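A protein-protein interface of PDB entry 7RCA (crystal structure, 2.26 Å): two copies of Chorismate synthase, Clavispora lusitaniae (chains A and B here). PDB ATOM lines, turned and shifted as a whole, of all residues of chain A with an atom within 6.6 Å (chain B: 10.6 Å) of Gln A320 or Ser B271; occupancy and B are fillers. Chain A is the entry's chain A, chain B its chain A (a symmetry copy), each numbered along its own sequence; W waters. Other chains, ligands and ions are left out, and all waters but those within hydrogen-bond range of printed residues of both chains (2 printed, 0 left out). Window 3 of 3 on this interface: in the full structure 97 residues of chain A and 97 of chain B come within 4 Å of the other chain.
The backbone carbonyl oxygen (O) of Ile B268 lies within hydrogen-bond range of the side-chain hydroxyl (OG) of Ser A314, at 2.7 Å.
The backbone NH (N) of Gly B270 is in hydrogen-bond range of the backbone carbonyl oxygen (O) of Ser A216.
OD2 of Asp A215 lies within hydrogen-bond range of OG of Ser B271.
The side-chain amide oxygen (OE1) of Gln A322 is in hydrogen-bond range of the side-chain amide nitrogen (ND2) of Asn B274 (3.0 Å).
The side-chain carboxylate of Asp A215 is in hydrogen-bond range of the backbone NH of Gly B270.
OG of Ser A216 lies within hydrogen-bond range of O of Ala A315, at 2.5 Å.
The backbone carbonyl oxygen of Ala A213 sits at hydrogen-bond distance from the side-chain amide nitrogen of Gln A320 (3.3 Å).
The backbone carbonyl oxygen of Gln A322 lies within hydrogen-bond range of the backbone NH of Leu A334, 2.7 Å away.
ND2 of Asn B274 lies close to O of Gly B270, at 3.4 Å.
Among the printed residues, merely in contact across the chains: Ser A216 with Pro B269, Asp A215 with Pro B269, Gln A320 with Ser B271 and Ser A314 with Gly B270.
Gln A320 touches just one residue of chain B: Ser B271.
Of the printed residues of chain A, Ser B271 touches Asp A215 (2.5 Å) and Gln A320 (3.6 Å).
Ser A216 touches two residues of chain B.
No residue of chain B comes within 4 Å of Ser A319.
Gln A322 touches one residue of chain B.
No residue of chain B comes within 4 Å of Ala A336.
Of the printed residues of chain A, Gly B270 touches Asp A215 (3.1 Å), Ser A216 (3.0 Å) and Ser A314 (3.9 Å).
Of the printed residues of chain A, Ile B268 touches Ser A314.
Printed residues of chain B within 4 Å of Asp A215: Pro B269, Gly B270 and Ser B271.
Of the printed residues of chain A, Asn B274 touches Gln A322.
His A340 touches none of the printed residues of chain B.
Arg B267 touches none of the printed residues of chain A.
The nearest residue of chain B that does not touch Gln A320 is Lys B272 (6.7 Å).
Of the 16 printed residues of chain B, 5 touch a printed residue of chain A.
Hydrophobic or aromatic side chains of chain B that line the printed part of chain A: Pro B269.
Among the printed residues, 9 pairs touch across the chains.
Among the printed residues, no Asp or Glu carboxylate lies within 4 Å of a Lys or Arg side-chain nitrogen of the other chain.
No position is printed for both chains.
Water W1 lies within hydrogen-bond range of O of Gly B265 (2.6 Å), N of Ser A314 (3.0 Å) and NE2 of His B273 (3.3 Å).
Water W2 bridges the side-chain amide nitrogen (NE2) of Gln A322 and the side-chain amide nitrogen (ND2) of Asn B274.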
ATOM      1  N   ALA A 213       4.882 -13.968  20.758  1.00  0.00           N
ATOM      2  CA  ALA A 213       4.337 -13.799  19.417  1.00  0.00           C
ATOM      3  C   ALA A 213       4.495 -15.044  18.557  1.00  0.00           C
ATOM      4  O   ALA A 213       4.026 -15.040  17.413  1.00  0.00           O
ATOM      5  CB  ALA A 213       5.001 -12.604  18.729  1.00  0.00           C
ATOM      6  N   LYS A 214       5.132 -16.096  19.078  1.00  0.00           N
ATOM      7  CA  LYS A 214       5.371 -17.333  18.336  1.00  0.00           C
ATOM      8  C   LYS A 214       6.114 -17.050  17.032  1.00  0.00           C
ATOM      9  O   LYS A 214       5.783 -17.588  15.972  1.00  0.00           O
ATOM     10  CB  LYS A 214       4.065 -18.086  18.075  1.00  0.00           C
ATOM     11  CG  LYS A 214       3.282 -18.430  19.340  1.00  0.00           C
ATOM     12  CD  LYS A 214       3.929 -19.577  20.105  1.00  0.00           C
ATOM     13  CE  LYS A 214       3.750 -19.419  21.611  1.00  0.00           C
ATOM     14  NZ  LYS A 214       4.774 -20.185  22.381  1.00  0.00           N
ATOM     15  N   ASP A 215       7.124 -16.194  17.113  1.00  0.00           N
ATOM     16  CA  ASP A 215       7.885 -15.730  15.965  1.00  0.00           C
ATOM     17  C   ASP A 215       9.362 -16.069  16.156  1.00  0.00           C
ATOM     18  O   ASP A 215       9.751 -16.732  17.121  1.00  0.00           O
ATOM     19  CB  ASP A 215       7.678 -14.224  15.763  1.00  0.00           C
ATOM     20  CG  ASP A 215       7.559 -13.843  14.301  1.00  0.00           C
ATOM     21  OD1 ASP A 215       8.248 -14.463  13.465  1.00  0.00           O
ATOM     22  OD2 ASP A 215       6.777 -12.918  13.988  1.00  0.00           O
ATOM     23  N   SER A 216      10.186 -15.602  15.220  1.00  0.00           N
ATOM     24  CA  SER A 216      11.628 -15.779  15.280  1.00  0.00           C
ATOM     25  C   SER A 216      12.295 -14.468  14.891  1.00  0.00           C
ATOM     26  O   SER A 216      11.713 -13.637  14.190  1.00  0.00           O
ATOM     27  CB  SER A 216      12.099 -16.908  14.357  1.00  0.00           C
ATOM     28  OG  SER A 216      11.978 -16.524  12.998  1.00  0.00           O
ATOM     29  N   SER A 314      16.528 -14.481  10.533  1.00  0.00           N
ATOM     30  CA  SER A 314      15.554 -15.050  11.451  1.00  0.00           C
ATOM     31  C   SER A 314      15.185 -16.459  11.007  1.00  0.00           C
ATOM     32  O   SER A 314      15.064 -16.736   9.811  1.00  0.00           O
ATOM     33  CB  SER A 314      14.305 -14.172  11.513  1.00  0.00           C
ATOM     34  OG  SER A 314      14.656 -12.801  11.544  1.00  0.00           O
ATOM     35  N   ALA A 315      15.014 -17.351  11.980  1.00  0.00           N
ATOM     36  CA  ALA A 315      14.734 -18.748  11.677  1.00  0.00           C
ATOM     37  C   ALA A 315      13.444 -18.877  10.877  1.00  0.00           C
ATOM     38  O   ALA A 315      12.427 -18.262  11.209  1.00  0.00           O
ATOM     39  CB  ALA A 315      14.642 -19.556  12.969  1.00  0.00           C
ATOM     40  N   THR A 317      11.705 -21.669  10.556  1.00  0.00           N
ATOM     41  CA  THR A 317      10.794 -22.515  11.320  1.00  0.00           C
ATOM     42  C   THR A 317      10.201 -21.690  12.453  1.00  0.00           C
ATOM     43  O   THR A 317      10.822 -21.514  13.505  1.00  0.00           O
ATOM     44  CB  THR A 317      11.523 -23.742  11.855  1.00  0.00           C
ATOM     45  OG1 THR A 317      12.026 -24.517  10.758  1.00  0.00           O
ATOM     46  CG2 THR A 317      10.574 -24.606  12.663  1.00  0.00           C
ATOM     47  N   ILE A 318       9.000 -21.167  12.237  1.00  0.00           N
ATOM     48  CA  ILE A 318       8.298 -20.374  13.236  1.00  0.00           C
ATOM     49  C   ILE A 318       7.160 -21.205  13.809  1.00  0.00           C
ATOM     50  O   ILE A 318       6.589 -22.072  13.137  1.00  0.00           O
ATOM     51  CB  ILE A 318       7.767 -19.045  12.655  1.00  0.00           C
ATOM     52  CG1 ILE A 318       6.834 -19.310  11.471  1.00  0.00           C
ATOM     53  CG2 ILE A 318       8.920 -18.134  12.254  1.00  0.00           C
ATOM     54  CD1 ILE A 318       6.132 -18.074  10.956  1.00  0.00           C
ATOM     55  N   SER A 319       6.835 -20.933  15.071  1.00  0.00           N
ATOM     56  CA  SER A 319       5.725 -21.594  15.743  1.00  0.00           C
ATOM     57  C   SER A 319       4.408 -20.921  15.377  1.00  0.00           C
ATOM     58  O   SER A 319       3.566 -20.669  16.245  1.00  0.00           O
ATOM     59  CB  SER A 319       5.941 -21.578  17.256  1.00  0.00           C
ATOM     60  OG  SER A 319       6.408 -20.316  17.693  1.00  0.00           O
ATOM     61  N   GLN A 320       4.218 -20.637  14.089  1.00  0.00           N
ATOM     62  CA  GLN A 320       3.105 -19.827  13.623  1.00  0.00           C
ATOM     63  C   GLN A 320       2.543 -20.420  12.339  1.00  0.00           C
ATOM     64  O   GLN A 320       3.157 -21.276  11.697  1.00  0.00           O
ATOM     65  CB  GLN A 320       3.539 -18.376  13.395  1.00  0.00           C
ATOM     66  CG  GLN A 320       2.500 -17.336  13.742  1.00  0.00           C
ATOM     67  CD  GLN A 320       2.928 -15.948  13.323  1.00  0.00           C
ATOM     68  OE1 GLN A 320       2.568 -15.473  12.246  1.00  0.00           O
ATOM     69  NE2 GLN A 320       3.716 -15.294  14.166  1.00  0.00           N
ATOM     70  N   GLU A 321       1.358 -19.946  11.971  1.00  0.00           N
ATOM     71  CA  GLU A 321       0.694 -20.359  10.744  1.00  0.00           C
ATOM     72  C   GLU A 321       1.170 -19.501   9.580  1.00  0.00           C
ATOM     73  O   GLU A 321       1.403 -18.299   9.732  1.00  0.00           O
ATOM     74  CB  GLU A 321      -0.824 -20.243  10.896  1.00  0.00           C
ATOM     75  CG  GLU A 321      -1.627 -21.053   9.893  1.00  0.00           C
ATOM     76  CD  GLU A 321      -3.120 -20.810  10.021  1.00  0.00           C
ATOM     77  OE1 GLU A 321      -3.876 -21.796  10.147  1.00  0.00           O
ATOM     78  OE2 GLU A 321      -3.536 -19.632   9.996  1.00  0.00           O
ATOM     79  N   GLN A 322       1.319 -20.128   8.414  1.00  0.00           N
ATOM     80  CA  GLN A 322       1.763 -19.432   7.216  1.00  0.00           C
ATOM     81  C   GLN A 322       0.910 -19.852   6.029  1.00  0.00           C
ATOM     82  O   GLN A 322       0.521 -21.018   5.915  1.00  0.00           O
ATOM     83  CB  GLN A 322       3.241 -19.712   6.914  1.00  0.00           C
ATOM     84  CG  GLN A 322       4.182 -19.486   8.085  1.00  0.00           C
ATOM     85  CD  GLN A 322       5.642 -19.486   7.667  1.00  0.00           C
ATOM     86  OE1 GLN A 322       6.164 -18.481   7.183  1.00  0.00           O
ATOM     87  NE2 GLN A 322       6.308 -20.619   7.851  1.00  0.00           N
ATOM     88  N   LEU A 334      -0.040 -23.621   6.178  1.00  0.00           N
ATOM     89  CA  LEU A 334       0.927 -24.466   6.869  1.00  0.00           C
ATOM     90  C   LEU A 334       0.718 -24.298   8.368  1.00  0.00           C
ATOM     91  O   LEU A 334       0.946 -23.214   8.917  1.00  0.00           O
ATOM     92  CB  LEU A 334       2.351 -24.098   6.462  1.00  0.00           C
ATOM     93  CG  LEU A 334       3.459 -24.952   7.077  1.00  0.00           C
ATOM     94  CD1 LEU A 334       3.398 -26.373   6.539  1.00  0.00           C
ATOM     95  CD2 LEU A 334       4.820 -24.335   6.809  1.00  0.00           C
ATOM     96  N   ALA A 335       0.279 -25.366   9.031  1.00  0.00           N
ATOM     97  CA  ALA A 335      -0.077 -25.281  10.440  1.00  0.00           C
ATOM     98  C   ALA A 335       1.142 -24.957  11.294  1.00  0.00           C
ATOM     99  O   ALA A 335       2.278 -25.307  10.961  1.00  0.00           O
ATOM    100  CB  ALA A 335      -0.711 -26.592  10.910  1.00  0.00           C
ATOM    101  N   ALA A 336       0.893 -24.271  12.407  1.00  0.00           N
ATOM    102  CA  ALA A 336       1.956 -23.914  13.335  1.00  0.00           C
ATOM    103  C   ALA A 336       2.514 -25.170  13.989  1.00  0.00           C
ATOM    104  O   ALA A 336       1.766 -25.951  14.586  1.00  0.00           O
ATOM    105  CB  ALA A 336       1.430 -22.950  14.395  1.00  0.00           C
ATOM    106  N   ARG A 337       3.828 -25.372  13.876  1.00  0.00           N
ATOM    107  CA  ARG A 337       4.436 -26.523  14.531  1.00  0.00           C
ATOM    108  C   ARG A 337       4.508 -26.315  16.039  1.00  0.00           C
ATOM    109  O   ARG A 337       4.221 -27.236  16.812  1.00  0.00           O
ATOM    110  CB  ARG A 337       5.825 -26.797  13.948  1.00  0.00           C
ATOM    111  CG  ARG A 337       5.910 -26.999  12.421  1.00  0.00           C
ATOM    112  CD  ARG A 337       4.776 -27.814  11.772  1.00  0.00           C
ATOM    113  NE  ARG A 337       4.171 -28.822  12.638  1.00  0.00           N
ATOM    114  CZ  ARG A 337       4.468 -30.114  12.615  1.00  0.00           C
ATOM    115  NH1 ARG A 337       5.378 -30.599  11.788  1.00  0.00           N
ATOM    116  NH2 ARG A 337       3.840 -30.938  13.448  1.00  0.00           N
ATOM    117  N   GLY A 338       4.785 -25.069  16.425  1.00  0.00           N
ATOM    118  CA  GLY A 338       4.823 -24.610  17.808  1.00  0.00           C
ATOM    119  C   GLY A 338       5.672 -25.208  18.911  1.00  0.00           C
ATOM    120  O   GLY A 338       5.152 -25.591  19.959  1.00  0.00           O
ATOM    121  N   HIS A 340       9.520 -24.129  18.905  1.00  0.00           N
ATOM    122  CA  HIS A 340      10.857 -23.675  18.547  1.00  0.00           C
ATOM    123  C   HIS A 340      11.230 -22.378  19.256  1.00  0.00           C
ATOM    124  O   HIS A 340      10.382 -21.517  19.509  1.00  0.00           O
ATOM    125  CB  HIS A 340      10.971 -23.488  17.033  1.00  0.00           C
ATOM    126  CG  HIS A 340      10.033 -24.355  16.256  1.00  0.00           C
ATOM    127  ND1 HIS A 340      10.311 -25.670  15.955  1.00  0.00           N
ATOM    128  CD2 HIS A 340       8.834 -24.084  15.686  1.00  0.00           C
ATOM    129  CE1 HIS A 340       9.319 -26.179  15.251  1.00  0.00           C
ATOM    130  NE2 HIS A 340       8.408 -25.238  15.073  1.00  0.00           N
ATOM    131  N   GLN B 170      12.818  -4.893   0.894  1.00  0.00           N
ATOM    132  CA  GLN B 170      11.365  -4.978   0.934  1.00  0.00           C
ATOM    133  C   GLN B 170      10.687  -3.872   0.137  1.00  0.00           C
ATOM    134  O   GLN B 170       9.480  -3.961  -0.113  1.00  0.00           O
ATOM    135  CB  GLN B 170      10.866  -4.942   2.384  1.00  0.00           C
ATOM    136  CG  GLN B 170      11.357  -6.100   3.244  1.00  0.00           C
ATOM    137  CD  GLN B 170      12.782  -5.911   3.726  1.00  0.00           C
ATOM    138  OE1 GLN B 170      13.090  -4.946   4.428  1.00  0.00           O
ATOM    139  NE2 GLN B 170      13.661  -6.834   3.353  1.00  0.00           N
ATOM    140  N   GLY B 265      18.073  -7.278   7.217  1.00  0.00           N
ATOM    141  CA  GLY B 265      16.997  -8.249   7.304  1.00  0.00           C
ATOM    142  C   GLY B 265      16.908  -8.954   8.640  1.00  0.00           C
ATOM    143  O   GLY B 265      15.849  -9.495   8.972  1.00  0.00           O
ATOM    144  N   THR B 266      17.995  -8.957   9.416  1.00  0.00           N
ATOM    145  CA  THR B 266      17.980  -9.577  10.734  1.00  0.00           C
ATOM    146  C   THR B 266      17.020  -8.891  11.695  1.00  0.00           C
ATOM    147  O   THR B 266      16.696  -9.468  12.738  1.00  0.00           O
ATOM    148  CB  THR B 266      19.390  -9.578  11.329  1.00  0.00           C
ATOM    149  OG1 THR B 266      19.834  -8.228  11.511  1.00  0.00           O
ATOM    150  CG2 THR B 266      20.356 -10.302  10.402  1.00  0.00           C
ATOM    151  N   ARG B 267      16.560  -7.684  11.372  1.00  0.00           N
ATOM    152  CA  ARG B 267      15.605  -6.959  12.196  1.00  0.00           C
ATOM    153  C   ARG B 267      14.157  -7.320  11.887  1.00  0.00           C
ATOM    154  O   ARG B 267      13.256  -6.838  12.580  1.00  0.00           O
ATOM    155  CB  ARG B 267      15.798  -5.450  12.015  1.00  0.00           C
ATOM    156  CG  ARG B 267      17.151  -4.938  12.481  1.00  0.00           C
ATOM    157  CD  ARG B 267      17.479  -3.600  11.839  1.00  0.00           C
ATOM    158  NE  ARG B 267      18.566  -2.918  12.531  1.00  0.00           N
ATOM    159  CZ  ARG B 267      18.437  -1.755  13.156  1.00  0.00           C
ATOM    160  NH1 ARG B 267      17.280  -1.116  13.195  1.00  0.00           N
ATOM    161  NH2 ARG B 267      19.495  -1.223  13.760  1.00  0.00           N
ATOM    162  N   ILE B 268      13.913  -8.146  10.880  1.00  0.00           N
ATOM    163  CA  ILE B 268      12.562  -8.499  10.448  1.00  0.00           C
ATOM    164  C   ILE B 268      12.216  -9.875  11.010  1.00  0.00           C
ATOM    165  O   ILE B 268      13.003 -10.815  10.832  1.00  0.00           O
ATOM    166  CB  ILE B 268      12.443  -8.494   8.915  1.00  0.00           C
ATOM    167  CG1 ILE B 268      12.949  -7.167   8.346  1.00  0.00           C
ATOM    168  CG2 ILE B 268      11.008  -8.761   8.481  1.00  0.00           C
ATOM    169  CD1 ILE B 268      13.196  -7.200   6.859  1.00  0.00           C
ATOM    170  N   PRO B 269      11.073 -10.036  11.675  1.00  0.00           N
ATOM    171  CA  PRO B 269      10.713 -11.348  12.219  1.00  0.00           C
ATOM    172  C   PRO B 269      10.411 -12.350  11.115  1.00  0.00           C
ATOM    173  O   PRO B 269      10.103 -11.992   9.975  1.00  0.00           O
ATOM    174  CB  PRO B 269       9.462 -11.064  13.062  1.00  0.00           C
ATOM    175  CG  PRO B 269       9.380  -9.572  13.182  1.00  0.00           C
ATOM    176  CD  PRO B 269      10.065  -9.011  11.983  1.00  0.00           C
ATOM    177  N   GLY B 270      10.492 -13.632  11.482  1.00  0.00           N
ATOM    178  CA  GLY B 270      10.306 -14.693  10.505  1.00  0.00           C
ATOM    179  C   GLY B 270       8.936 -14.689   9.856  1.00  0.00           C
ATOM    180  O   GLY B 270       8.795 -15.088   8.697  1.00  0.00           O
ATOM    181  N   SER B 271       7.911 -14.240  10.584  1.00  0.00           N
ATOM    182  CA  SER B 271       6.563 -14.193  10.025  1.00  0.00           C
ATOM    183  C   SER B 271       6.484 -13.266   8.820  1.00  0.00           C
ATOM    184  O   SER B 271       5.680 -13.499   7.909  1.00  0.00           O
ATOM    185  CB  SER B 271       5.568 -13.748  11.097  1.00  0.00           C
ATOM    186  OG  SER B 271       5.986 -12.534  11.694  1.00  0.00           O
ATOM    187  N   LYS B 272       7.296 -12.211   8.797  1.00  0.00           N
ATOM    188  CA  LYS B 272       7.368 -11.307   7.657  1.00  0.00           C
ATOM    189  C   LYS B 272       8.577 -11.564   6.774  1.00  0.00           C
ATOM    190  O   LYS B 272       8.515 -11.317   5.565  1.00  0.00           O
ATOM    191  CB  LYS B 272       7.399  -9.849   8.135  1.00  0.00           C
ATOM    192  CG  LYS B 272       6.512  -9.562   9.341  1.00  0.00           C
ATOM    193  CD  LYS B 272       6.082  -8.102   9.376  1.00  0.00           C
ATOM    194  CE  LYS B 272       5.136  -7.822  10.539  1.00  0.00           C
ATOM    195  NZ  LYS B 272       5.284  -8.825  11.634  1.00  0.00           N
ATOM    196  N   HIS B 273       9.672 -12.061   7.348  1.00  0.00           N
ATOM    197  CA  HIS B 273      10.878 -12.294   6.566  1.00  0.00           C
ATOM    198  C   HIS B 273      10.762 -13.531   5.683  1.00  0.00           C
ATOM    199  O   HIS B 273      11.410 -13.596   4.633  1.00  0.00           O
ATOM    200  CB  HIS B 273      12.085 -12.416   7.495  1.00  0.00           C
ATOM    201  CG  HIS B 273      13.390 -12.537   6.775  1.00  0.00           C
ATOM    202  ND1 HIS B 273      13.933 -13.752   6.419  1.00  0.00           N
ATOM    203  CD2 HIS B 273      14.257 -11.593   6.336  1.00  0.00           C
ATOM    204  CE1 HIS B 273      15.081 -13.554   5.796  1.00  0.00           C
ATOM    205  NE2 HIS B 273      15.300 -12.253   5.732  1.00  0.00           N
ATOM    206  N   ASN B 274       9.947 -14.506   6.077  1.00  0.00           N
ATOM    207  CA  ASN B 274       9.821 -15.736   5.309  1.00  0.00           C
ATOM    208  C   ASN B 274       9.195 -15.469   3.944  1.00  0.00           C
ATOM    209  O   ASN B 274       8.323 -14.609   3.790  1.00  0.00           O
ATOM    210  CB  ASN B 274       8.982 -16.762   6.070  1.00  0.00           C
ATOM    211  CG  ASN B 274       9.794 -17.539   7.087  1.00  0.00           C
ATOM    212  OD1 ASN B 274      11.013 -17.386   7.169  1.00  0.00           O
ATOM    213  ND2 ASN B 274       9.119 -18.370   7.875  1.00  0.00           N
ATOM    214  N   ASP B 275       9.651 -16.227   2.946  1.00  0.00           N
ATOM    215  CA  ASP B 275       9.179 -16.078   1.578  1.00  0.00           C
ATOM    216  C   ASP B 275       8.178 -17.178   1.262  1.00  0.00           C
ATOM    217  O   ASP B 275       8.586 -18.336   1.075  1.00  0.00           O
ATOM    218  CB  ASP B 275      10.353 -16.129   0.602  1.00  0.00           C
ATOM    219  CG  ASP B 275      11.344 -15.000   0.824  1.00  0.00           C
ATOM    220  OD1 ASP B 275      10.896 -13.856   1.053  1.00  0.00           O
ATOM    221  OD2 ASP B 275      12.569 -15.256   0.769  1.00  0.00           O
ATOM    222  N   PRO B 276       6.882 -16.884   1.188  1.00  0.00           N
ATOM    223  CA  PRO B 276       5.912 -17.930   0.844  1.00  0.00           C
ATOM    224  C   PRO B 276       6.029 -18.339  -0.616  1.00  0.00           C
ATOM    225  O   PRO B 276       6.472 -17.567  -1.470  1.00  0.00           O
ATOM    226  CB  PRO B 276       4.554 -17.269   1.124  1.00  0.00           C
ATOM    227  CG  PRO B 276       4.862 -16.014   1.898  1.00  0.00           C
ATOM    228  CD  PRO B 276       6.231 -15.597   1.471  1.00  0.00           C
ATOM    229  N   LYS B 289       6.651 -15.649  -3.312  1.00  0.00           N
ATOM    230  CA  LYS B 289       5.963 -14.360  -3.304  1.00  0.00           C
ATOM    231  C   LYS B 289       6.944 -13.215  -3.081  1.00  0.00           C
ATOM    232  O   LYS B 289       6.963 -12.240  -3.843  1.00  0.00           O
ATOM    233  CB  LYS B 289       4.873 -14.354  -2.233  1.00  0.00           C
ATOM    234  CG  LYS B 289       3.481 -14.067  -2.764  1.00  0.00           C
ATOM    235  CD  LYS B 289       2.411 -14.433  -1.746  1.00  0.00           C
ATOM    236  CE  LYS B 289       1.826 -15.808  -2.031  1.00  0.00           C
ATOM    237  NZ  LYS B 289       1.149 -16.386  -0.839  1.00  0.00           N
ATOM    238  N   THR B 290       7.760 -13.315  -2.038  1.00  0.00           N
ATOM    239  CA  THR B 290       8.822 -12.362  -1.755  1.00  0.00           C
ATOM    240  C   THR B 290      10.173 -13.042  -1.942  1.00  0.00           C
ATOM    241  O   THR B 290      10.267 -14.274  -2.010  1.00  0.00           O
ATOM    242  CB  THR B 290       8.704 -11.801  -0.332  1.00  0.00           C
ATOM    243  OG1 THR B 290       8.619 -12.882   0.608  1.00  0.00           O
ATOM    244  CG2 THR B 290       7.460 -10.929  -0.204  1.00  0.00           C
ATOM    245  N   ASN B 292      13.169 -12.354   0.051  1.00  0.00           N
ATOM    246  CA  ASN B 292      14.101 -12.015   1.118  1.00  0.00           C
ATOM    247  C   ASN B 292      15.277 -12.980   1.160  1.00  0.00           C
ATOM    248  O   ASN B 292      16.367 -12.608   1.611  1.00  0.00           O
ATOM    249  CB  ASN B 292      13.381 -11.994   2.465  1.00  0.00           C
ATOM    250  CG  ASN B 292      12.551 -10.746   2.652  1.00  0.00           C
ATOM    251  OD1 ASN B 292      13.016  -9.637   2.390  1.00  0.00           O
ATOM    252  ND2 ASN B 292      11.315 -10.917   3.115  1.00  0.00           N
HETATM  253  O   HOH W   1      16.363 -12.059   8.798  1.00  0.00           O
HETATM  254  O   HOH W   2       8.833 -21.712   7.300  1.00  0.00           O
